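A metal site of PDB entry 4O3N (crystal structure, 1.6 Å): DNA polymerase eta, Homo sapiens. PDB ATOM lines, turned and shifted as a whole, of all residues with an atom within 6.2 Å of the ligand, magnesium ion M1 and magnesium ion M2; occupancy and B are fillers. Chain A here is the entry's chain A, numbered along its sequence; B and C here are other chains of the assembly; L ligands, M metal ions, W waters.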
ATOM      1  N   ASP A  16     -10.772 -13.923  25.888  1.00  0.00           N
ATOM      2  CA  ASP A  16      -9.478 -13.268  25.631  1.00  0.00           C
ATOM      3  C   ASP A  16      -9.457 -12.758  24.214  1.00  0.00           C
ATOM      4  O   ASP A  16      -9.645 -13.519  23.271  1.00  0.00           O
ATOM      5  CB  ASP A  16      -8.298 -14.216  25.840  1.00  0.00           C
ATOM      6  CG  ASP A  16      -6.989 -13.518  25.679  1.00  0.00           C
ATOM      7  OD1 ASP A  16      -6.431 -13.109  26.684  1.00  0.00           O
ATOM      8  OD2 ASP A  16      -6.580 -13.346  24.559  1.00  0.00           O
ATOM      9  N   MET A  17      -9.165 -11.490  24.053  1.00  0.00           N
ATOM     10  CA  MET A  17      -9.210 -10.960  22.715  1.00  0.00           C
ATOM     11  C   MET A  17      -8.096 -11.502  21.806  1.00  0.00           C
ATOM     12  O   MET A  17      -7.003 -11.742  22.247  1.00  0.00           O
ATOM     13  CB  MET A  17      -9.063  -9.422  22.737  1.00  0.00           C
ATOM     14  CG  MET A  17     -10.129  -8.737  23.653  1.00  0.00           C
ATOM     15  SD  MET A  17     -11.849  -9.101  23.302  1.00  0.00           S
ATOM     16  CE  MET A  17     -12.022  -8.472  21.711  1.00  0.00           C
ATOM     17  N   ASP A  18      -8.432 -11.691  20.553  1.00  0.00           N
ATOM     18  CA  ASP A  18      -7.420 -12.171  19.588  1.00  0.00           C
ATOM     19  C   ASP A  18      -6.503 -11.004  19.205  1.00  0.00           C
ATOM     20  O   ASP A  18      -7.003  -9.900  18.942  1.00  0.00           O
ATOM     21  CB  ASP A  18      -8.071 -12.808  18.369  1.00  0.00           C
ATOM     22  CG  ASP A  18      -8.933 -14.038  18.727  1.00  0.00           C
ATOM     23  OD1 ASP A  18      -8.634 -14.727  19.717  1.00  0.00           O
ATOM     24  OD2 ASP A  18      -9.863 -14.317  18.003  1.00  0.00           O
ATOM     25  N   CYS A  19      -5.202 -11.279  19.190  1.00  0.00           N
ATOM     26  CA  CYS A  19      -4.127 -10.319  18.835  1.00  0.00           C
ATOM     27  C   CYS A  19      -4.597  -8.890  19.100  1.00  0.00           C
ATOM     28  O   CYS A  19      -4.707  -8.072  18.189  1.00  0.00           O
ATOM     29  CB  CYS A  19      -3.648 -10.490  17.382  1.00  0.00           C
ATOM     30  SG  CYS A  19      -4.881 -10.510  16.056  1.00  0.00           S
ATOM     31  N   PHE A  20      -4.855  -8.595  20.377  1.00  0.00           N
ATOM     32  CA  PHE A  20      -5.720  -7.451  20.697  1.00  0.00           C
ATOM     33  C   PHE A  20      -5.213  -6.118  20.141  1.00  0.00           C
ATOM     34  O   PHE A  20      -5.971  -5.453  19.477  1.00  0.00           O
ATOM     35  CB  PHE A  20      -5.876  -7.336  22.198  1.00  0.00           C
ATOM     36  CG  PHE A  20      -6.854  -6.277  22.631  1.00  0.00           C
ATOM     37  CD1 PHE A  20      -8.065  -6.099  21.969  1.00  0.00           C
ATOM     38  CD2 PHE A  20      -6.520  -5.404  23.654  1.00  0.00           C
ATOM     39  CE1 PHE A  20      -8.978  -5.123  22.367  1.00  0.00           C
ATOM     40  CE2 PHE A  20      -7.459  -4.391  24.063  1.00  0.00           C
ATOM     41  CZ  PHE A  20      -8.648  -4.281  23.395  1.00  0.00           C
ATOM     42  N   PHE A  21      -3.969  -5.731  20.441  1.00  0.00           N
ATOM     43  CA  PHE A  21      -3.542  -4.385  20.020  1.00  0.00           C
ATOM     44  C   PHE A  21      -3.505  -4.308  18.494  1.00  0.00           C
ATOM     45  O   PHE A  21      -3.833  -3.282  17.949  1.00  0.00           O
ATOM     46  CB  PHE A  21      -2.164  -3.978  20.538  1.00  0.00           C
ATOM     47  CG  PHE A  21      -2.090  -3.723  22.007  1.00  0.00           C
ATOM     48  CD1 PHE A  21      -3.130  -4.081  22.882  1.00  0.00           C
ATOM     49  CD2 PHE A  21      -0.930  -3.165  22.529  1.00  0.00           C
ATOM     50  CE1 PHE A  21      -3.013  -3.806  24.266  1.00  0.00           C
ATOM     51  CE2 PHE A  21      -0.813  -2.850  23.899  1.00  0.00           C
ATOM     52  CZ  PHE A  21      -1.883  -3.231  24.775  1.00  0.00           C
ATOM     53  N   VAL A  22      -3.201  -5.413  17.813  1.00  0.00           N
ATOM     54  CA  VAL A  22      -3.282  -5.426  16.348  1.00  0.00           C
ATOM     55  C   VAL A  22      -4.738  -5.173  15.914  1.00  0.00           C
ATOM     56  O   VAL A  22      -4.967  -4.395  14.993  1.00  0.00           O
ATOM     57  CB  VAL A  22      -2.747  -6.724  15.807  1.00  0.00           C
ATOM     58  CG1 VAL A  22      -3.142  -6.935  14.317  1.00  0.00           C
ATOM     59  CG2 VAL A  22      -1.237  -6.786  15.990  1.00  0.00           C
ATOM     60  N   ILE A  51       5.111  -5.731  20.211  1.00  0.00           N
ATOM     61  CA  ILE A  51       4.333  -6.130  21.417  1.00  0.00           C
ATOM     62  C   ILE A  51       3.034  -6.866  21.034  1.00  0.00           C
ATOM     63  O   ILE A  51       2.389  -7.448  21.916  1.00  0.00           O
ATOM     64  CB  ILE A  51       4.020  -4.966  22.303  1.00  0.00           C
ATOM     65  CG1 ILE A  51       3.073  -3.954  21.652  1.00  0.00           C
ATOM     66  CG2 ILE A  51       5.364  -4.352  22.825  1.00  0.00           C
ATOM     67  CD1 ILE A  51       2.725  -2.816  22.587  1.00  0.00           C
ATOM     68  N   ALA A  52       2.681  -6.935  19.754  1.00  0.00           N
ATOM     69  CA  ALA A  52       1.503  -7.741  19.338  1.00  0.00           C
ATOM     70  C   ALA A  52       1.642  -8.092  17.884  1.00  0.00           C
ATOM     71  O   ALA A  52       2.199  -7.287  17.116  1.00  0.00           O
ATOM     72  CB  ALA A  52       0.167  -6.955  19.593  1.00  0.00           C
ATOM     73  N   VAL A  53       1.094  -9.262  17.482  1.00  0.00           N
ATOM     74  CA  VAL A  53       1.362  -9.839  16.186  1.00  0.00           C
ATOM     75  C   VAL A  53       0.102 -10.437  15.609  1.00  0.00           C
ATOM     76  O   VAL A  53      -0.527 -11.297  16.280  1.00  0.00           O
ATOM     77  CB  VAL A  53       2.459 -10.958  16.310  1.00  0.00           C
ATOM     78  CG1 VAL A  53       2.937 -11.401  14.917  1.00  0.00           C
ATOM     79  CG2 VAL A  53       3.638 -10.439  17.108  1.00  0.00           C
ATOM     80  N   TYR A  55      -2.264 -12.944  13.292  1.00  0.00           N
ATOM     81  CA  TYR A  55      -2.063 -14.358  12.983  1.00  0.00           C
ATOM     82  C   TYR A  55      -1.409 -14.565  11.639  1.00  0.00           C
ATOM     83  O   TYR A  55      -0.590 -15.488  11.557  1.00  0.00           O
ATOM     84  CB  TYR A  55      -3.401 -15.145  13.117  1.00  0.00           C
ATOM     85  CG  TYR A  55      -3.734 -15.378  14.571  1.00  0.00           C
ATOM     86  CD1 TYR A  55      -4.301 -14.366  15.344  1.00  0.00           C
ATOM     87  CD2 TYR A  55      -3.350 -16.545  15.216  1.00  0.00           C
ATOM     88  CE1 TYR A  55      -4.505 -14.544  16.712  1.00  0.00           C
ATOM     89  CE2 TYR A  55      -3.533 -16.732  16.579  1.00  0.00           C
ATOM     90  CZ  TYR A  55      -4.126 -15.751  17.334  1.00  0.00           C
ATOM     91  OH  TYR A  55      -4.356 -15.947  18.687  1.00  0.00           O
ATOM     92  N   ARG A  58       2.239 -14.270  12.476  1.00  0.00           N
ATOM     93  CA  ARG A  58       2.721 -15.425  13.278  1.00  0.00           C
ATOM     94  C   ARG A  58       3.127 -16.608  12.371  1.00  0.00           C
ATOM     95  O   ARG A  58       4.054 -17.362  12.757  1.00  0.00           O
ATOM     96  CB  ARG A  58       1.663 -15.897  14.284  1.00  0.00           C
ATOM     97  CG  ARG A  58       1.347 -14.847  15.286  1.00  0.00           C
ATOM     98  CD  ARG A  58       0.292 -15.305  16.303  1.00  0.00           C
ATOM     99  NE  ARG A  58      -0.271 -14.125  16.985  1.00  0.00           N
ATOM    100  CZ  ARG A  58      -0.961 -14.155  18.115  1.00  0.00           C
ATOM    101  NH1 ARG A  58      -1.196 -15.320  18.725  1.00  0.00           N
ATOM    102  NH2 ARG A  58      -1.419 -12.989  18.625  1.00  0.00           N
ATOM    103  N   ARG A  64       6.118 -11.669  19.620  1.00  0.00           N
ATOM    104  CA  ARG A  64       6.364 -10.626  20.587  1.00  0.00           C
ATOM    105  C   ARG A  64       7.808 -10.645  21.060  1.00  0.00           C
ATOM    106  O   ARG A  64       8.474 -11.708  21.089  1.00  0.00           O
ATOM    107  CB  ARG A  64       5.395 -10.759  21.769  1.00  0.00           C
ATOM    108  CG  ARG A  64       5.553  -9.793  22.866  1.00  0.00           C
ATOM    109  CD  ARG A  64       4.841 -10.344  24.093  1.00  0.00           C
ATOM    110  NE  ARG A  64       3.473 -10.703  23.775  1.00  0.00           N
ATOM    111  CZ  ARG A  64       2.931 -11.909  23.972  1.00  0.00           C
ATOM    112  NH1 ARG A  64       3.624 -12.921  24.493  1.00  0.00           N
ATOM    113  NH2 ARG A  64       1.642 -12.081  23.657  1.00  0.00           N
ATOM    114  N   LEU A  92      -0.332   4.095  26.284  1.00  0.00           N
ATOM    115  CA  LEU A  92      -1.221   2.970  25.936  1.00  0.00           C
ATOM    116  C   LEU A  92      -2.719   3.310  25.991  1.00  0.00           C
ATOM    117  O   LEU A  92      -3.570   2.402  25.955  1.00  0.00           O
ATOM    118  CB  LEU A  92      -0.896   1.797  26.865  1.00  0.00           C
ATOM    119  CG  LEU A  92       0.531   1.326  26.755  1.00  0.00           C
ATOM    120  CD1 LEU A  92       0.678   0.324  27.843  1.00  0.00           C
ATOM    121  CD2 LEU A  92       0.745   0.703  25.343  1.00  0.00           C
ATOM    122  N   SER A 116      -6.834  -8.791  32.664  1.00  0.00           N
ATOM    123  CA  SER A 116      -5.761  -8.084  31.964  1.00  0.00           C
ATOM    124  C   SER A 116      -6.415  -7.032  31.081  1.00  0.00           C
ATOM    125  O   SER A 116      -7.624  -6.921  31.022  1.00  0.00           O
ATOM    126  CB  SER A 116      -4.934  -9.021  31.075  1.00  0.00           C
ATOM    127  OG  SER A 116      -5.623  -9.358  29.834  1.00  0.00           O
ATOM    128  N   ILE A 117      -5.601  -6.338  30.271  1.00  0.00           N
ATOM    129  CA  ILE A 117      -6.204  -5.363  29.352  1.00  0.00           C
ATOM    130  C   ILE A 117      -7.144  -6.020  28.306  1.00  0.00           C
ATOM    131  O   ILE A 117      -8.020  -5.351  27.745  1.00  0.00           O
ATOM    132  CB  ILE A 117      -5.089  -4.532  28.665  1.00  0.00           C
ATOM    133  CG1 ILE A 117      -5.649  -3.254  28.080  1.00  0.00           C
ATOM    134  CG2 ILE A 117      -4.360  -5.378  27.591  1.00  0.00           C
ATOM    135  CD1 ILE A 117      -4.500  -2.282  27.709  1.00  0.00           C
ATOM    136  N   ASP A 118      -6.941  -7.329  28.064  1.00  0.00           N
ATOM    137  CA  ASP A 118      -7.721  -7.939  27.000  1.00  0.00           C
ATOM    138  C   ASP A 118      -8.444  -9.210  27.418  1.00  0.00           C
ATOM    139  O   ASP A 118      -8.906  -9.944  26.547  1.00  0.00           O
ATOM    140  CB  ASP A 118      -6.857  -8.191  25.744  1.00  0.00           C
ATOM    141  CG  ASP A 118      -6.183  -9.585  25.741  1.00  0.00           C
ATOM    142  OD1 ASP A 118      -5.717 -10.077  26.817  1.00  0.00           O
ATOM    143  OD2 ASP A 118      -6.260 -10.225  24.658  1.00  0.00           O
ATOM    144  N   GLU A 119      -8.594  -9.443  28.720  1.00  0.00           N
ATOM    145  CA  GLU A 119      -9.381 -10.620  29.115  1.00  0.00           C
ATOM    146  C   GLU A 119     -10.081 -10.472  30.407  1.00  0.00           C
ATOM    147  O   GLU A 119      -9.692  -9.648  31.265  1.00  0.00           O
ATOM    148  CB  GLU A 119      -8.545 -11.859  29.175  1.00  0.00           C
ATOM    149  CG  GLU A 119      -7.559 -11.904  30.267  1.00  0.00           C
ATOM    150  CD  GLU A 119      -6.320 -12.678  29.855  1.00  0.00           C
ATOM    151  OE1 GLU A 119      -5.484 -12.122  29.123  1.00  0.00           O
ATOM    152  OE2 GLU A 119      -6.173 -13.871  30.229  1.00  0.00           O
ATOM    153  N   LYS A 227      -9.153 -20.738  31.346  1.00  0.00           N
ATOM    154  CA  LYS A 227      -8.052 -20.066  30.702  1.00  0.00           C
ATOM    155  C   LYS A 227      -7.321 -21.030  29.767  1.00  0.00           C
ATOM    156  O   LYS A 227      -7.007 -20.678  28.640  1.00  0.00           O
ATOM    157  CB  LYS A 227      -7.053 -19.500  31.747  1.00  0.00           C
ATOM    158  CG  LYS A 227      -5.802 -18.865  31.154  1.00  0.00           C
ATOM    159  CD  LYS A 227      -6.162 -17.637  30.245  1.00  0.00           C
ATOM    160  CE  LYS A 227      -4.832 -16.845  29.936  1.00  0.00           C
ATOM    161  NZ  LYS A 227      -4.809 -15.809  28.835  1.00  0.00           N
ATOM    162  N   LYS A 234      -7.779 -20.926  19.784  1.00  0.00           N
ATOM    163  CA  LYS A 234      -7.615 -19.542  19.355  1.00  0.00           C
ATOM    164  C   LYS A 234      -7.041 -19.580  17.933  1.00  0.00           C
ATOM    165  O   LYS A 234      -6.156 -20.436  17.674  1.00  0.00           O
ATOM    166  CB  LYS A 234      -6.655 -18.878  20.353  1.00  0.00           C
ATOM    167  CG  LYS A 234      -6.800 -17.478  20.650  1.00  0.00           C
ATOM    168  CD  LYS A 234      -5.846 -17.058  21.712  1.00  0.00           C
ATOM    169  CE  LYS A 234      -6.594 -16.156  22.707  1.00  0.00           C
ATOM    170  NZ  LYS A 234      -7.117 -14.849  22.057  1.00  0.00           N
ATOM    171  N   PRO A 235      -7.420 -18.651  17.019  1.00  0.00           N
ATOM    172  CA  PRO A 235      -8.285 -17.478  17.269  1.00  0.00           C
ATOM    173  C   PRO A 235      -9.741 -17.704  16.825  1.00  0.00           C
ATOM    174  O   PRO A 235     -10.080 -18.629  16.046  1.00  0.00           O
ATOM    175  CB  PRO A 235      -7.656 -16.376  16.398  1.00  0.00           C
ATOM    176  CG  PRO A 235      -7.241 -17.157  15.099  1.00  0.00           C
ATOM    177  CD  PRO A 235      -6.817 -18.572  15.665  1.00  0.00           C
ATOM    178  P    DT B   8      -0.198 -14.768  30.738  1.00  0.00           P
ATOM    179  OP1  DT B   8      -1.270 -15.687  30.274  1.00  0.00           O
ATOM    180  OP2  DT B   8       1.216 -14.870  30.272  1.00  0.00           O
ATOM    181  O5'  DT B   8      -0.665 -13.270  30.438  1.00  0.00           O
ATOM    182  C5'  DT B   8      -1.953 -12.851  30.762  1.00  0.00           C
ATOM    183  C4'  DT B   8      -2.098 -11.469  30.230  1.00  0.00           C
ATOM    184  O4'  DT B   8      -0.996 -10.710  30.750  1.00  0.00           O
ATOM    185  C3'  DT B   8      -2.014 -11.388  28.700  1.00  0.00           C
ATOM    186  O3'  DT B   8      -3.102 -10.576  28.219  1.00  0.00           O
ATOM    187  C2'  DT B   8      -0.634 -10.765  28.442  1.00  0.00           C
ATOM    188  C1'  DT B   8      -0.383  -9.975  29.703  1.00  0.00           C
ATOM    189  N1   DT B   8       1.056  -9.840  30.038  1.00  0.00           N
ATOM    190  C2   DT B   8       1.615  -8.579  30.091  1.00  0.00           C
ATOM    191  O2   DT B   8       0.984  -7.572  29.831  1.00  0.00           O
ATOM    192  N3   DT B   8       2.941  -8.555  30.441  1.00  0.00           N
ATOM    193  C4   DT B   8       3.738  -9.645  30.706  1.00  0.00           C
ATOM    194  O4   DT B   8       4.921  -9.545  30.999  1.00  0.00           O
ATOM    195  C5   DT B   8       3.100 -10.929  30.605  1.00  0.00           C
ATOM    196  C7   DT B   8       3.873 -12.170  30.896  1.00  0.00           C
ATOM    197  C6   DT B   8       1.799 -10.962  30.287  1.00  0.00           C
ATOM    198  P    DT C   3      17.500  -7.214  25.216  1.00  0.00           P
ATOM    199  OP1  DT C   3      18.286  -7.743  26.357  1.00  0.00           O
ATOM    200  OP2  DT C   3      17.450  -7.851  23.868  1.00  0.00           O
ATOM    201  O5'  DT C   3      16.026  -7.109  25.783  1.00  0.00           O
ATOM    202  C5'  DT C   3      14.931  -7.455  24.957  1.00  0.00           C
ATOM    203  C4'  DT C   3      14.027  -6.265  24.879  1.00  0.00           C
ATOM    204  O4'  DT C   3      12.750  -6.630  24.303  1.00  0.00           O
ATOM    205  C3'  DT C   3      13.691  -5.637  26.244  1.00  0.00           C
ATOM    206  O3'  DT C   3      14.146  -4.330  26.286  1.00  0.00           O
ATOM    207  C2'  DT C   3      12.164  -5.658  26.302  1.00  0.00           C
ATOM    208  C1'  DT C   3      11.856  -5.661  24.823  1.00  0.00           C
ATOM    209  N1   DT C   3      10.502  -6.059  24.533  1.00  0.00           N
ATOM    210  C2   DT C   3       9.696  -5.198  23.801  1.00  0.00           C
ATOM    211  O2   DT C   3      10.097  -4.113  23.324  1.00  0.00           O
ATOM    212  N3   DT C   3       8.451  -5.649  23.629  1.00  0.00           N
ATOM    213  C4   DT C   3       7.906  -6.844  24.123  1.00  0.00           C
ATOM    214  O4   DT C   3       6.744  -7.171  23.911  1.00  0.00           O
ATOM    215  C5   DT C   3       8.781  -7.669  24.899  1.00  0.00           C
ATOM    216  C7   DT C   3       8.282  -8.975  25.475  1.00  0.00           C
ATOM    217  C6   DT C   3      10.026  -7.241  25.071  1.00  0.00           C
ATOM    218  P    DG C   4      13.740  -3.426  27.533  1.00  0.00           P
ATOM    219  OP1  DG C   4      14.581  -2.210  27.505  1.00  0.00           O
ATOM    220  OP2  DG C   4      13.440  -4.324  28.667  1.00  0.00           O
ATOM    221  O5'  DG C   4      12.278  -2.889  27.185  1.00  0.00           O
ATOM    222  C5'  DG C   4      12.076  -1.910  26.222  1.00  0.00           C
ATOM    223  C4'  DG C   4      10.700  -1.308  26.462  1.00  0.00           C
ATOM    224  O4'  DG C   4       9.641  -2.326  26.408  1.00  0.00           O
ATOM    225  C3'  DG C   4      10.530  -0.637  27.803  1.00  0.00           C
ATOM    226  O3'  DG C   4       9.662   0.473  27.579  1.00  0.00           O
ATOM    227  C2'  DG C   4       9.881  -1.711  28.665  1.00  0.00           C
ATOM    228  C1'  DG C   4       8.942  -2.363  27.631  1.00  0.00           C
ATOM    229  N9   DG C   4       8.676  -3.755  27.880  1.00  0.00           N
ATOM    230  C8   DG C   4       9.470  -4.737  28.400  1.00  0.00           C
ATOM    231  N7   DG C   4       8.886  -5.924  28.427  1.00  0.00           N
ATOM    232  C5   DG C   4       7.618  -5.671  27.877  1.00  0.00           C
ATOM    233  C6   DG C   4       6.557  -6.542  27.613  1.00  0.00           C
ATOM    234  O6   DG C   4       6.465  -7.752  27.885  1.00  0.00           O
ATOM    235  N1   DG C   4       5.475  -5.863  27.028  1.00  0.00           N
ATOM    236  C2   DG C   4       5.444  -4.518  26.722  1.00  0.00           C
ATOM    237  N2   DG C   4       4.286  -4.029  26.187  1.00  0.00           N
ATOM    238  N3   DG C   4       6.456  -3.688  26.951  1.00  0.00           N
ATOM    239  C4   DG C   4       7.513  -4.359  27.503  1.00  0.00           C
ATOM    240  P    DA C   5       9.198   1.491  28.713  1.00  0.00           P
ATOM    241  OP1  DA C   5       9.294   2.829  28.154  1.00  0.00           O
ATOM    242  OP2  DA C   5       9.922   1.175  29.968  1.00  0.00           O
ATOM    243  O5'  DA C   5       7.679   1.063  29.021  1.00  0.00           O
ATOM    244  C5'  DA C   5       6.692   1.348  28.054  1.00  0.00           C
ATOM    245  C4'  DA C   5       5.344   0.941  28.586  1.00  0.00           C
ATOM    246  O4'  DA C   5       5.313  -0.502  28.661  1.00  0.00           O
ATOM    247  C3'  DA C   5       4.993   1.468  29.966  1.00  0.00           C
ATOM    248  O3'  DA C   5       3.599   1.757  29.988  1.00  0.00           O
ATOM    249  C2'  DA C   5       5.300   0.263  30.884  1.00  0.00           C
ATOM    250  C1'  DA C   5       4.870  -0.893  29.944  1.00  0.00           C
ATOM    251  N9   DA C   5       5.443  -2.190  30.250  1.00  0.00           N
ATOM    252  C8   DA C   5       6.719  -2.463  30.694  1.00  0.00           C
ATOM    253  N7   DA C   5       6.941  -3.727  30.924  1.00  0.00           N
ATOM    254  C5   DA C   5       5.755  -4.352  30.556  1.00  0.00           C
ATOM    255  C6   DA C   5       5.351  -5.679  30.631  1.00  0.00           C
ATOM    256  N6   DA C   5       6.160  -6.686  31.039  1.00  0.00           N
ATOM    257  N1   DA C   5       4.087  -5.947  30.237  1.00  0.00           N
ATOM    258  C2   DA C   5       3.284  -4.939  29.866  1.00  0.00           C
ATOM    259  N3   DA C   5       3.547  -3.651  29.790  1.00  0.00           N
ATOM    260  C4   DA C   5       4.813  -3.420  30.182  1.00  0.00           C
HETATM  261  P1  LIG L   1      -3.723 -13.757  21.367  1.00  0.00           P
HETATM  262  O1  LIG L   1      -4.410 -13.546  22.688  1.00  0.00           O
HETATM  263  O2  LIG L   1      -2.651 -14.872  21.446  1.00  0.00           O
HETATM  264  O3  LIG L   1      -4.647 -13.933  20.230  1.00  0.00           O
HETATM  265  P2  LIG L   1      -2.800 -11.078  22.029  1.00  0.00           P
HETATM  266  O4  LIG L   1      -4.186 -10.641  22.450  1.00  0.00           O
HETATM  267  O5  LIG L   1      -1.994 -10.075  21.252  1.00  0.00           O
HETATM  268  O6  LIG L   1      -2.908 -12.363  21.096  1.00  0.00           O
HETATM  269  P3  LIG L   1      -2.350 -11.480  24.946  1.00  0.00           P
HETATM  270  O7  LIG L   1      -1.274 -12.222  25.719  1.00  0.00           O
HETATM  271  O8  LIG L   1      -3.739 -11.838  25.238  1.00  0.00           O
HETATM  272  N1  LIG L   1      -1.900 -11.637  23.324  1.00  0.00           N
HETATM  273  O9  LIG L   1      -2.074  -9.954  25.303  1.00  0.00           O
HETATM  274  C1  LIG L   1      -3.029  -8.911  25.026  1.00  0.00           C
HETATM  275  C2  LIG L   1      -2.384  -7.671  24.600  1.00  0.00           C
HETATM  276  O10 LIG L   1      -1.472  -7.204  25.746  1.00  0.00           O
HETATM  277  C3  LIG L   1      -1.397  -7.748  23.418  1.00  0.00           C
HETATM  278  O11 LIG L   1      -2.127  -7.557  22.155  1.00  0.00           O
HETATM  279  C4  LIG L   1      -0.476  -6.725  23.650  1.00  0.00           C
HETATM  280  C5  LIG L   1      -0.344  -6.646  25.247  1.00  0.00           C
HETATM  281  N2  LIG L   1       0.788  -7.373  25.725  1.00  0.00           N
HETATM  282  C6  LIG L   1       1.933  -6.613  26.077  1.00  0.00           C
HETATM  283  N3  LIG L   1       3.022  -7.343  26.627  1.00  0.00           N
HETATM  284  C7  LIG L   1       2.986  -8.716  26.789  1.00  0.00           C
HETATM  285  C8  LIG L   1       1.803  -9.471  26.475  1.00  0.00           C
HETATM  286  C9  LIG L   1       0.705  -8.745  25.935  1.00  0.00           C
HETATM  287  O12 LIG L   1       1.971  -5.375  25.858  1.00  0.00           O
HETATM  288  N4  LIG L   1       4.117  -9.343  27.352  1.00  0.00           N
HETATM  289 MG    MG M   1      -4.802 -11.998  27.186  1.00  0.00          MG
HETATM  290 MG    MG M   2      -5.365 -11.907  23.724  1.00  0.00          MG
HETATM  291  O   HOH W   1      -0.178 -14.274  22.260  1.00  0.00           O
HETATM  292  O   HOH W   2       3.874 -12.269  27.216  1.00  0.00           O
HETATM  293  O   HOH W   3      -3.643 -13.807  27.102  1.00  0.00           O
HETATM  294  O   HOH W   4      -3.950 -15.276  24.795  1.00  0.00           O
HETATM  295  O   HOH W   5      -0.600  -5.730  28.564  1.00  0.00           O
HETATM  296  O   HOH W   6       1.374  -2.989  26.435  1.00  0.00           O
HETATM  297  O   HOH W   7       0.081 -10.691  19.746  1.00  0.00           O
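Residues that only touch the ligand: Asp 18 (3.3 Å), Ile 51 (3.4 Å), Ala 52 (3.5 Å) and Ile 117 (3.9 Å).
Hydrophobic or aromatic side chains within 4 Å of the ligand: Phe 20, Phe 21, Ala 52, Tyr 55 and Ile 117.
16 residues have an atom within 4 Å of the ligand: Asp 16, Met 17, Asp 18, Cys 19, Phe 20, Phe 21, Ile 51, Ala 52, Tyr 55, Arg 58, Arg 64, Ile 117, Asp 118, Lys 234, DT 8 of chain B and DG 4 of chain C.
The nearest printed residue that does not touch the ligand is DA 5 of chain C (4.01 Å).
N3 of DT 8 of chain B lies close to a nitrogen (N4) of the ligand (3.4 Å).
The side-chain hydroxyl of Tyr 55 lies within hydrogen-bond range of an oxygen (O3) of the ligand, at 2.6 Å.
O6 of DG 4 of chain C lies within hydrogen-bond range of a nitrogen (N4) of the ligand (2.9 Å).
An oxygen (O3) of the ligand lies within hydrogen-bond range of the backbone NH (N) of Cys 19, 2.9 Å away.
An oxygen (O2) of the ligand is in salt-bridge range of the guanidinium group of Arg 58 (3.1 Å).
The backbone NH of Phe 20 sits at hydrogen-bond distance from an oxygen (O5) of the ligand (3.3 Å).
The side-chain amino group (NZ) of Lys 234 lies within salt-bridge range of an oxygen (O3) of the ligand (3.2 Å).
N of Phe 21 sits at hydrogen-bond distance from O11 of the ligand (3.1 Å).
The guanidinium group (NH2) of Arg 64 is in salt-bridge range of an oxygen (O7) of the ligand (3.6 Å).
Residues that only touch magnesium ion M2: Lys 234 (3.8 Å).
Of the 25 residues printed, 4 come within 4 Å of magnesium ion M2.
Along chain A the residues within 4 Å of magnesium ion M2 span positions 16 to 234.
The nearest printed residue that does not touch magnesium ion M2 is Asp 18 (4.4 Å).
Magnesium ion M2 is bound by the side-chain carboxylate of Asp 16 (2.1 Å), the side-chain carboxylate of Asp 118 (2.1 Å), an oxygen (O4) of the ligand (2.1 Å), an oxygen (O1) of the ligand (2.2 Å), the backbone carbonyl oxygen of Met 17 (2.2 Å) and an oxygen (O8) of the ligand (2.2 Å).
Magnesium ion M2 has six donor atoms within binding distance.
Water W3 lies within hydrogen-bond range of the side-chain amino group of Lys 227 (2.9 Å) and an oxygen (O7) of the ligand (3.2 Å).
Water W6 bridges O12 of the ligand (2.5 Å) and N2 of DG 4 of chain C (3.1 Å).
Water W7 lies within hydrogen-bond range of an oxygen (O5) of the ligand (2.6 Å), the backbone NH (N) of Val 53 (2.9 Å) and the guanidinium group (NH2) of Arg 58 (3.0 Å).
Water W1 bridges an oxygen (O2) of the ligand (2.7 Å) and the guanidinium group of Arg 64 (3.2 Å).
Water W2 lies within hydrogen-bond range of NH1 of Arg 64 (2.8 Å) and N4 of the ligand (2.9 Å).
Water W5 bridges O2 of DT 8 of chain B (2.7 Å) and O10 of the ligand (3.3 Å).
The backbone carbonyl oxygen of Asp 16 lies within hydrogen-bond range of the side-chain amino group of Lys 234 (3.1 Å).
The side-chain hydroxyl (OG) of Ser 116 lies within hydrogen-bond range of the backbone NH (N) of Glu 119 (3.2 Å).
The side-chain carboxylate of Glu 119 is in salt-bridge range of the side-chain amino group of Lys 227, at 2.7 Å.
The backbone NH of Asp 118 is in hydrogen-bond range of the side-chain hydroxyl of Ser 116 (3.0 Å).
The side-chain amino group (NZ) of Lys 234 lies close to the backbone carbonyl oxygen (O) of Met 17 (3.1 Å).
OG of Ser 116 sits close to O3' of DT 8 of chain B (3.2 Å).
O of Val 53 is in hydrogen-bond range of NE of Arg 58, 2.9 Å away.
The side-chain amino group of Lys 234 is in salt-bridge range of the side-chain carboxylate of Asp 18 (2.8 Å).
Magnesium ion M1 is bound by the side-chain carboxylate (OD1) of Asp 16 (2.0 Å), the side-chain carboxylate (OE1) of Glu 119 (2.1 Å), water W3 (2.2 Å), the side-chain carboxylate (OD1) of Asp 118 (2.2 Å), an oxygen (O8) of the ligand (2.2 Å) and O3' of DT 8 of chain B (2.4 Å).
Residues that only touch magnesium ion M1: Ser 116.
Within 4 Å of magnesium ion M1: Asp 16, Ser 116, Asp 118, Glu 119 and DT 8 of chain B.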
